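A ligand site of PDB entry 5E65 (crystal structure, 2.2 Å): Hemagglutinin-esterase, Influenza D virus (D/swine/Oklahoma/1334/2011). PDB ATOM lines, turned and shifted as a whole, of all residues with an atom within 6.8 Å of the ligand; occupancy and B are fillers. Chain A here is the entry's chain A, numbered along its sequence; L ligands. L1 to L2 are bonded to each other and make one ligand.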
ATOM      1  N   PHE A 125       3.940 -20.903   3.446  1.00  0.00           N
ATOM      2  CA  PHE A 125       4.341 -22.245   2.991  1.00  0.00           C
ATOM      3  C   PHE A 125       3.153 -23.179   2.724  1.00  0.00           C
ATOM      4  O   PHE A 125       3.328 -24.386   2.629  1.00  0.00           O
ATOM      5  CB  PHE A 125       5.276 -22.915   4.010  1.00  0.00           C
ATOM      6  CG  PHE A 125       6.535 -22.148   4.272  1.00  0.00           C
ATOM      7  CD1 PHE A 125       7.212 -21.522   3.251  1.00  0.00           C
ATOM      8  CD2 PHE A 125       7.040 -22.067   5.564  1.00  0.00           C
ATOM      9  CE1 PHE A 125       8.384 -20.817   3.505  1.00  0.00           C
ATOM     10  CE2 PHE A 125       8.200 -21.361   5.825  1.00  0.00           C
ATOM     11  CZ  PHE A 125       8.872 -20.736   4.796  1.00  0.00           C
ATOM     12  N   THR A 166      13.898 -21.698  19.159  1.00  0.00           N
ATOM     13  CA  THR A 166      13.277 -20.387  19.197  1.00  0.00           C
ATOM     14  C   THR A 166      12.109 -20.275  18.221  1.00  0.00           C
ATOM     15  O   THR A 166      11.945 -21.120  17.339  1.00  0.00           O
ATOM     16  CB  THR A 166      14.298 -19.277  18.884  1.00  0.00           C
ATOM     17  OG1 THR A 166      14.964 -19.574  17.656  1.00  0.00           O
ATOM     18  CG2 THR A 166      15.326 -19.168  20.000  1.00  0.00           C
ATOM     19  N   ALA A 167      11.298 -19.230  18.375  1.00  0.00           N
ATOM     20  CA  ALA A 167      10.083 -19.057  17.591  1.00  0.00           C
ATOM     21  C   ALA A 167      10.367 -18.835  16.101  1.00  0.00           C
ATOM     22  O   ALA A 167      11.278 -18.105  15.744  1.00  0.00           O
ATOM     23  CB  ALA A 167       9.262 -17.898  18.146  1.00  0.00           C
ATOM     24  N   GLY A 168       9.564 -19.465  15.252  1.00  0.00           N
ATOM     25  CA  GLY A 168       9.779 -19.434  13.816  1.00  0.00           C
ATOM     26  C   GLY A 168       9.191 -18.241  13.068  1.00  0.00           C
ATOM     27  O   GLY A 168       8.123 -17.749  13.411  1.00  0.00           O
ATOM     28  N   THR A 169       9.911 -17.802  12.039  1.00  0.00           N
ATOM     29  CA  THR A 169       9.503 -16.650  11.237  1.00  0.00           C
ATOM     30  C   THR A 169       9.782 -16.931   9.756  1.00  0.00           C
ATOM     31  O   THR A 169      10.783 -17.556   9.422  1.00  0.00           O
ATOM     32  CB  THR A 169      10.239 -15.381  11.691  1.00  0.00           C
ATOM     33  OG1 THR A 169       9.570 -14.831  12.834  1.00  0.00           O
ATOM     34  CG2 THR A 169      10.288 -14.320  10.590  1.00  0.00           C
ATOM     35  N   ALA A 170       8.882 -16.487   8.881  1.00  0.00           N
ATOM     36  CA  ALA A 170       9.062 -16.718   7.447  1.00  0.00           C
ATOM     37  C   ALA A 170       8.681 -15.523   6.588  1.00  0.00           C
ATOM     38  O   ALA A 170       7.639 -14.898   6.805  1.00  0.00           O
ATOM     39  CB  ALA A 170       8.263 -17.939   7.018  1.00  0.00           C
ATOM     40  N   SER A 171       9.518 -15.233   5.594  1.00  0.00           N
ATOM     41  CA  SER A 171       9.254 -14.160   4.636  1.00  0.00           C
ATOM     42  C   SER A 171       7.918 -14.362   3.909  1.00  0.00           C
ATOM     43  O   SER A 171       7.280 -13.395   3.516  1.00  0.00           O
ATOM     44  CB  SER A 171      10.383 -14.090   3.595  1.00  0.00           C
ATOM     45  OG  SER A 171      10.491 -15.320   2.887  1.00  0.00           O
ATOM     46  N   SER A 172       7.486 -15.615   3.771  1.00  0.00           N
ATOM     47  CA  SER A 172       6.249 -15.943   3.089  1.00  0.00           C
ATOM     48  C   SER A 172       5.040 -15.743   3.985  1.00  0.00           C
ATOM     49  O   SER A 172       3.892 -15.797   3.516  1.00  0.00           O
ATOM     50  CB  SER A 172       6.298 -17.369   2.571  1.00  0.00           C
ATOM     51  OG  SER A 172       6.439 -18.297   3.631  1.00  0.00           O
ATOM     52  N   SER A 175       6.749 -12.078   7.399  1.00  0.00           N
ATOM     53  CA  SER A 175       7.895 -12.048   8.303  1.00  0.00           C
ATOM     54  C   SER A 175       7.478 -12.360   9.732  1.00  0.00           C
ATOM     55  O   SER A 175       8.003 -11.795  10.685  1.00  0.00           O
ATOM     56  CB  SER A 175       8.604 -10.687   8.226  1.00  0.00           C
ATOM     57  OG  SER A 175       8.954 -10.361   6.899  1.00  0.00           O
ATOM     58  N   TRP A 177       4.503 -15.496  11.804  1.00  0.00           N
ATOM     59  CA  TRP A 177       3.974 -16.845  11.727  1.00  0.00           C
ATOM     60  C   TRP A 177       2.527 -16.941  12.247  1.00  0.00           C
ATOM     61  O   TRP A 177       2.021 -16.022  12.886  1.00  0.00           O
ATOM     62  CB  TRP A 177       4.879 -17.817  12.486  1.00  0.00           C
ATOM     63  CG  TRP A 177       4.543 -19.240  12.195  1.00  0.00           C
ATOM     64  CD1 TRP A 177       4.107 -20.182  13.080  1.00  0.00           C
ATOM     65  CD2 TRP A 177       4.585 -19.883  10.918  1.00  0.00           C
ATOM     66  NE1 TRP A 177       3.879 -21.374  12.432  1.00  0.00           N
ATOM     67  CE2 TRP A 177       4.166 -21.210  11.102  1.00  0.00           C
ATOM     68  CE3 TRP A 177       4.940 -19.451   9.636  1.00  0.00           C
ATOM     69  CZ2 TRP A 177       4.101 -22.122  10.043  1.00  0.00           C
ATOM     70  CZ3 TRP A 177       4.874 -20.355   8.588  1.00  0.00           C
ATOM     71  CH2 TRP A 177       4.460 -21.678   8.805  1.00  0.00           C
ATOM     72  N   TRP A 183       5.732 -22.511  15.717  1.00  0.00           N
ATOM     73  CA  TRP A 183       6.883 -22.964  14.956  1.00  0.00           C
ATOM     74  C   TRP A 183       8.157 -22.791  15.774  1.00  0.00           C
ATOM     75  O   TRP A 183       8.506 -21.673  16.136  1.00  0.00           O
ATOM     76  CB  TRP A 183       6.980 -22.193  13.650  1.00  0.00           C
ATOM     77  CG  TRP A 183       8.006 -22.702  12.690  1.00  0.00           C
ATOM     78  CD1 TRP A 183       8.694 -23.874  12.760  1.00  0.00           C
ATOM     79  CD2 TRP A 183       8.466 -22.033  11.506  1.00  0.00           C
ATOM     80  NE1 TRP A 183       9.548 -23.986  11.690  1.00  0.00           N
ATOM     81  CE2 TRP A 183       9.434 -22.867  10.904  1.00  0.00           C
ATOM     82  CE3 TRP A 183       8.150 -20.817  10.890  1.00  0.00           C
ATOM     83  CZ2 TRP A 183      10.078 -22.531   9.720  1.00  0.00           C
ATOM     84  CZ3 TRP A 183       8.799 -20.472   9.725  1.00  0.00           C
ATOM     85  CH2 TRP A 183       9.754 -21.324   9.146  1.00  0.00           C
ATOM     86  N   TYR A 184       8.830 -23.891  16.074  1.00  0.00           N
ATOM     87  CA  TYR A 184      10.075 -23.825  16.838  1.00  0.00           C
ATOM     88  C   TYR A 184      11.249 -24.375  16.037  1.00  0.00           C
ATOM     89  O   TYR A 184      11.197 -25.480  15.505  1.00  0.00           O
ATOM     90  CB  TYR A 184       9.931 -24.593  18.150  1.00  0.00           C
ATOM     91  CG  TYR A 184       9.023 -23.905  19.147  1.00  0.00           C
ATOM     92  CD1 TYR A 184       9.496 -22.872  19.941  1.00  0.00           C
ATOM     93  CD2 TYR A 184       7.703 -24.294  19.280  1.00  0.00           C
ATOM     94  CE1 TYR A 184       8.666 -22.238  20.857  1.00  0.00           C
ATOM     95  CE2 TYR A 184       6.867 -23.675  20.190  1.00  0.00           C
ATOM     96  CZ  TYR A 184       7.351 -22.644  20.976  1.00  0.00           C
ATOM     97  OH  TYR A 184       6.515 -22.025  21.886  1.00  0.00           O
ATOM     98  N   ALA A 185      12.316 -23.586  15.967  1.00  0.00           N
ATOM     99  CA  ALA A 185      13.466 -23.939  15.149  1.00  0.00           C
ATOM    100  C   ALA A 185      14.766 -23.934  15.943  1.00  0.00           C
ATOM    101  O   ALA A 185      14.983 -23.099  16.817  1.00  0.00           O
ATOM    102  CB  ALA A 185      13.568 -22.989  13.965  1.00  0.00           C
ATOM    103  N   PHE A 227       5.693 -30.567   7.787  1.00  0.00           N
ATOM    104  CA  PHE A 227       6.267 -29.980   6.597  1.00  0.00           C
ATOM    105  C   PHE A 227       6.409 -31.018   5.488  1.00  0.00           C
ATOM    106  O   PHE A 227       6.673 -32.190   5.752  1.00  0.00           O
ATOM    107  CB  PHE A 227       7.620 -29.344   6.908  1.00  0.00           C
ATOM    108  CG  PHE A 227       7.498 -28.070   7.680  1.00  0.00           C
ATOM    109  CD1 PHE A 227       6.882 -26.960   7.126  1.00  0.00           C
ATOM    110  CD2 PHE A 227       8.010 -27.969   8.965  1.00  0.00           C
ATOM    111  CE1 PHE A 227       6.778 -25.780   7.836  1.00  0.00           C
ATOM    112  CE2 PHE A 227       7.917 -26.796   9.681  1.00  0.00           C
ATOM    113  CZ  PHE A 227       7.290 -25.701   9.112  1.00  0.00           C
ATOM    114  N   TYR A 229       8.407 -31.992   2.053  1.00  0.00           N
ATOM    115  CA  TYR A 229       9.549 -31.835   1.150  1.00  0.00           C
ATOM    116  C   TYR A 229       9.353 -32.806  -0.010  1.00  0.00           C
ATOM    117  O   TYR A 229       8.605 -33.768   0.111  1.00  0.00           O
ATOM    118  CB  TYR A 229      10.846 -32.109   1.880  1.00  0.00           C
ATOM    119  CG  TYR A 229      11.049 -31.212   3.079  1.00  0.00           C
ATOM    120  CD1 TYR A 229      11.830 -30.068   2.990  1.00  0.00           C
ATOM    121  CD2 TYR A 229      10.429 -31.502   4.291  1.00  0.00           C
ATOM    122  CE1 TYR A 229      11.990 -29.240   4.080  1.00  0.00           C
ATOM    123  CE2 TYR A 229      10.589 -30.674   5.381  1.00  0.00           C
ATOM    124  CZ  TYR A 229      11.376 -29.555   5.267  1.00  0.00           C
ATOM    125  OH  TYR A 229      11.549 -28.715   6.347  1.00  0.00           O
ATOM    126  N   PHE A 235      15.416 -32.361   1.533  1.00  0.00           N
ATOM    127  CA  PHE A 235      15.271 -32.123   2.980  1.00  0.00           C
ATOM    128  C   PHE A 235      16.614 -31.976   3.660  1.00  0.00           C
ATOM    129  O   PHE A 235      16.769 -31.182   4.589  1.00  0.00           O
ATOM    130  CB  PHE A 235      14.494 -33.244   3.663  1.00  0.00           C
ATOM    131  CG  PHE A 235      14.420 -33.073   5.154  1.00  0.00           C
ATOM    132  CD1 PHE A 235      13.584 -32.120   5.705  1.00  0.00           C
ATOM    133  CD2 PHE A 235      15.186 -33.859   6.007  1.00  0.00           C
ATOM    134  CE1 PHE A 235      13.516 -31.937   7.071  1.00  0.00           C
ATOM    135  CE2 PHE A 235      15.112 -33.681   7.378  1.00  0.00           C
ATOM    136  CZ  PHE A 235      14.271 -32.724   7.908  1.00  0.00           C
ATOM    137  N   PHE A 238      18.338 -28.961   4.976  1.00  0.00           N
ATOM    138  CA  PHE A 238      18.027 -28.392   6.293  1.00  0.00           C
ATOM    139  C   PHE A 238      18.313 -29.333   7.463  1.00  0.00           C
ATOM    140  O   PHE A 238      18.867 -28.910   8.471  1.00  0.00           O
ATOM    141  CB  PHE A 238      16.566 -27.954   6.346  1.00  0.00           C
ATOM    142  CG  PHE A 238      16.242 -26.776   5.475  1.00  0.00           C
ATOM    143  CD1 PHE A 238      16.629 -25.493   5.855  1.00  0.00           C
ATOM    144  CD2 PHE A 238      15.552 -26.931   4.288  1.00  0.00           C
ATOM    145  CE1 PHE A 238      16.336 -24.400   5.057  1.00  0.00           C
ATOM    146  CE2 PHE A 238      15.247 -25.846   3.486  1.00  0.00           C
ATOM    147  CZ  PHE A 238      15.639 -24.575   3.876  1.00  0.00           C
ATOM    148  N   VAL A 273       9.664 -26.059   0.098  1.00  0.00           N
ATOM    149  CA  VAL A 273       9.032 -26.533   1.324  1.00  0.00           C
ATOM    150  C   VAL A 273       7.565 -26.115   1.385  1.00  0.00           C
ATOM    151  O   VAL A 273       7.210 -24.973   1.089  1.00  0.00           O
ATOM    152  CB  VAL A 273       9.774 -26.014   2.584  1.00  0.00           C
ATOM    153  CG1 VAL A 273       9.830 -24.488   2.603  1.00  0.00           C
ATOM    154  CG2 VAL A 273       9.128 -26.553   3.851  1.00  0.00           C
ATOM    155  N   ARG A 294      15.784 -29.775  13.691  1.00  0.00           N
ATOM    156  CA  ARG A 294      15.720 -28.361  13.357  1.00  0.00           C
ATOM    157  C   ARG A 294      14.297 -27.766  13.417  1.00  0.00           C
ATOM    158  O   ARG A 294      14.134 -26.637  13.872  1.00  0.00           O
ATOM    159  CB  ARG A 294      16.314 -28.099  11.962  1.00  0.00           C
ATOM    160  CG  ARG A 294      16.111 -26.666  11.512  1.00  0.00           C
ATOM    161  CD  ARG A 294      17.125 -26.198  10.504  1.00  0.00           C
ATOM    162  NE  ARG A 294      17.192 -24.732  10.498  1.00  0.00           N
ATOM    163  CZ  ARG A 294      17.994 -24.024   9.711  1.00  0.00           C
ATOM    164  NH1 ARG A 294      18.793 -24.627   8.860  1.00  0.00           N
ATOM    165  NH2 ARG A 294      17.985 -22.696   9.781  1.00  0.00           N
ATOM    166  N   PHE A 295      13.300 -28.519  12.983  1.00  0.00           N
ATOM    167  CA  PHE A 295      11.945 -27.969  12.921  1.00  0.00           C
ATOM    168  C   PHE A 295      10.942 -28.735  13.773  1.00  0.00           C
ATOM    169  O   PHE A 295      10.888 -29.965  13.733  1.00  0.00           O
ATOM    170  CB  PHE A 295      11.467 -27.914  11.465  1.00  0.00           C
ATOM    171  CG  PHE A 295      12.253 -26.970  10.616  1.00  0.00           C
ATOM    172  CD1 PHE A 295      12.624 -25.725  11.094  1.00  0.00           C
ATOM    173  CD2 PHE A 295      12.632 -27.317   9.328  1.00  0.00           C
ATOM    174  CE1 PHE A 295      13.348 -24.842  10.315  1.00  0.00           C
ATOM    175  CE2 PHE A 295      13.363 -26.451   8.535  1.00  0.00           C
ATOM    176  CZ  PHE A 295      13.720 -25.209   9.034  1.00  0.00           C
HETATM  177  C1  LIG L   1      15.549 -19.134   1.795  1.00  0.00           C
HETATM  178  C2  LIG L   1      15.777 -18.592   3.183  1.00  0.00           C
HETATM  179  C3  LIG L   1      14.569 -17.903   3.656  1.00  0.00           C
HETATM  180  C4  LIG L   1      13.997 -16.915   2.691  1.00  0.00           C
HETATM  181  C5  LIG L   1      14.026 -17.405   1.263  1.00  0.00           C
HETATM  182  C6  LIG L   1      13.989 -16.236   0.326  1.00  0.00           C
HETATM  183  O1  LIG L   1      16.755 -19.721   1.288  1.00  0.00           O
HETATM  184  O2  LIG L   1      16.002 -19.640   4.104  1.00  0.00           O
HETATM  185  O3  LIG L   1      14.878 -17.210   4.843  1.00  0.00           O
HETATM  186  O4  LIG L   1      14.633 -15.703   2.893  1.00  0.00           O
HETATM  187  O5  LIG L   1      15.234 -18.022   0.973  1.00  0.00           O
HETATM  188  O6  LIG L   1      13.023 -16.483  -0.684  1.00  0.00           O
HETATM  189  C1  LG2 L   2      10.505 -24.056   7.028  1.00  0.00           C
HETATM  190  C2  LG2 L   2      11.641 -24.389   6.133  1.00  0.00           C
HETATM  191  C3  LG2 L   2      12.421 -20.358  11.513  1.00  0.00           C
HETATM  192  C4  LG2 L   2      13.287 -20.269  10.282  1.00  0.00           C
HETATM  193  C5  LG2 L   2      13.296 -22.979   6.142  1.00  0.00           C
HETATM  194  C6  LG2 L   2      13.400 -21.517   5.945  1.00  0.00           C
HETATM  195  C7  LG2 L   2      13.324 -20.892   7.306  1.00  0.00           C
HETATM  196  N1  LG2 L   2      13.254 -19.107   9.642  1.00  0.00           N
HETATM  197  C8  LG2 L   2      14.013 -18.774   8.455  1.00  0.00           C
HETATM  198  C9  LG2 L   2      13.817 -17.295   8.272  1.00  0.00           C
HETATM  199  C10 LG2 L   2      13.417 -19.390   7.255  1.00  0.00           C
HETATM  200  C11 LG2 L   2      14.472 -16.756   7.059  1.00  0.00           C
HETATM  201  C12 LG2 L   2      14.021 -17.527   5.901  1.00  0.00           C
HETATM  202  C13 LG2 L   2      12.586 -17.186   5.577  1.00  0.00           C
HETATM  203  O1  LG2 L   2      11.998 -25.535   5.997  1.00  0.00           O
HETATM  204  O2  LG2 L   2      12.149 -23.356   5.491  1.00  0.00           O
HETATM  205  O3  LG2 L   2      13.918 -21.237   9.913  1.00  0.00           O
HETATM  206  O4  LG2 L   2      14.348 -21.430   8.086  1.00  0.00           O
HETATM  207  O5  LG2 L   2      12.265 -21.195   5.236  1.00  0.00           O
HETATM  208  O6  LG2 L   2      14.327 -16.628   9.343  1.00  0.00           O
HETATM  209  O7  LG2 L   2      14.108 -18.906   6.121  1.00  0.00           O
HETATM  210  O8  LG2 L   2      11.917 -18.090   5.089  1.00  0.00           O
HETATM  211  O9  LG2 L   2      12.216 -16.028   5.756  1.00  0.00           O
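The backbone carbonyl oxygen (O) of Thr 169 is in hydrogen-bond range of a nitrogen (N1) of LG2 L2, 2.9 Å away. An oxygen (O9) of LG2 L2 sits at hydrogen-bond distance from the side-chain hydroxyl (OG) of Ser 171, at 3.4 Å. An oxygen (O9) of LG2 L2 is in hydrogen-bond range of the backbone NH (N) of Ser 171 (2.8 Å). OH of Tyr 229 lies within hydrogen-bond range of O1 of LG2 L2, at 3.2 Å.
The backbone NH of Ala 185 is in hydrogen-bond range of the backbone carbonyl oxygen of Thr 166 (2.8 Å). N of Gly 168 sits at hydrogen-bond distance from O of Trp 183 (2.6 Å). O of Ala 170 sits at hydrogen-bond distance from N of Ser 175 (3.0 Å).
CZ of Phe 125 touches O5 of LG2 L2, 3.5 Å away. Gly 168 touches the ligand. CA of Ala 170 touches O9 of LG2 L2, at 3.6 Å. CZ2 of Trp 183 touches C1 of LG2 L2, at 3.1 Å. CB of Ala 185 touches C3 of LG2 L2, 3.8 Å away. Phe 238 touches the ligand. Val 273 touches the ligand. CE2 of Phe 295 touches O1 of LG2 L2, 3.0 Å away. Hydrophobic or aromatic side chains that line the ligand: Phe 125, Trp 183, Ala 185, Phe 238, Val 273 and Phe 295. Of the 20 residues printed, 11 come within 4 Å of the ligand. The nearest printed residue that does not touch the ligand is Phe 227 (4.2 Å).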
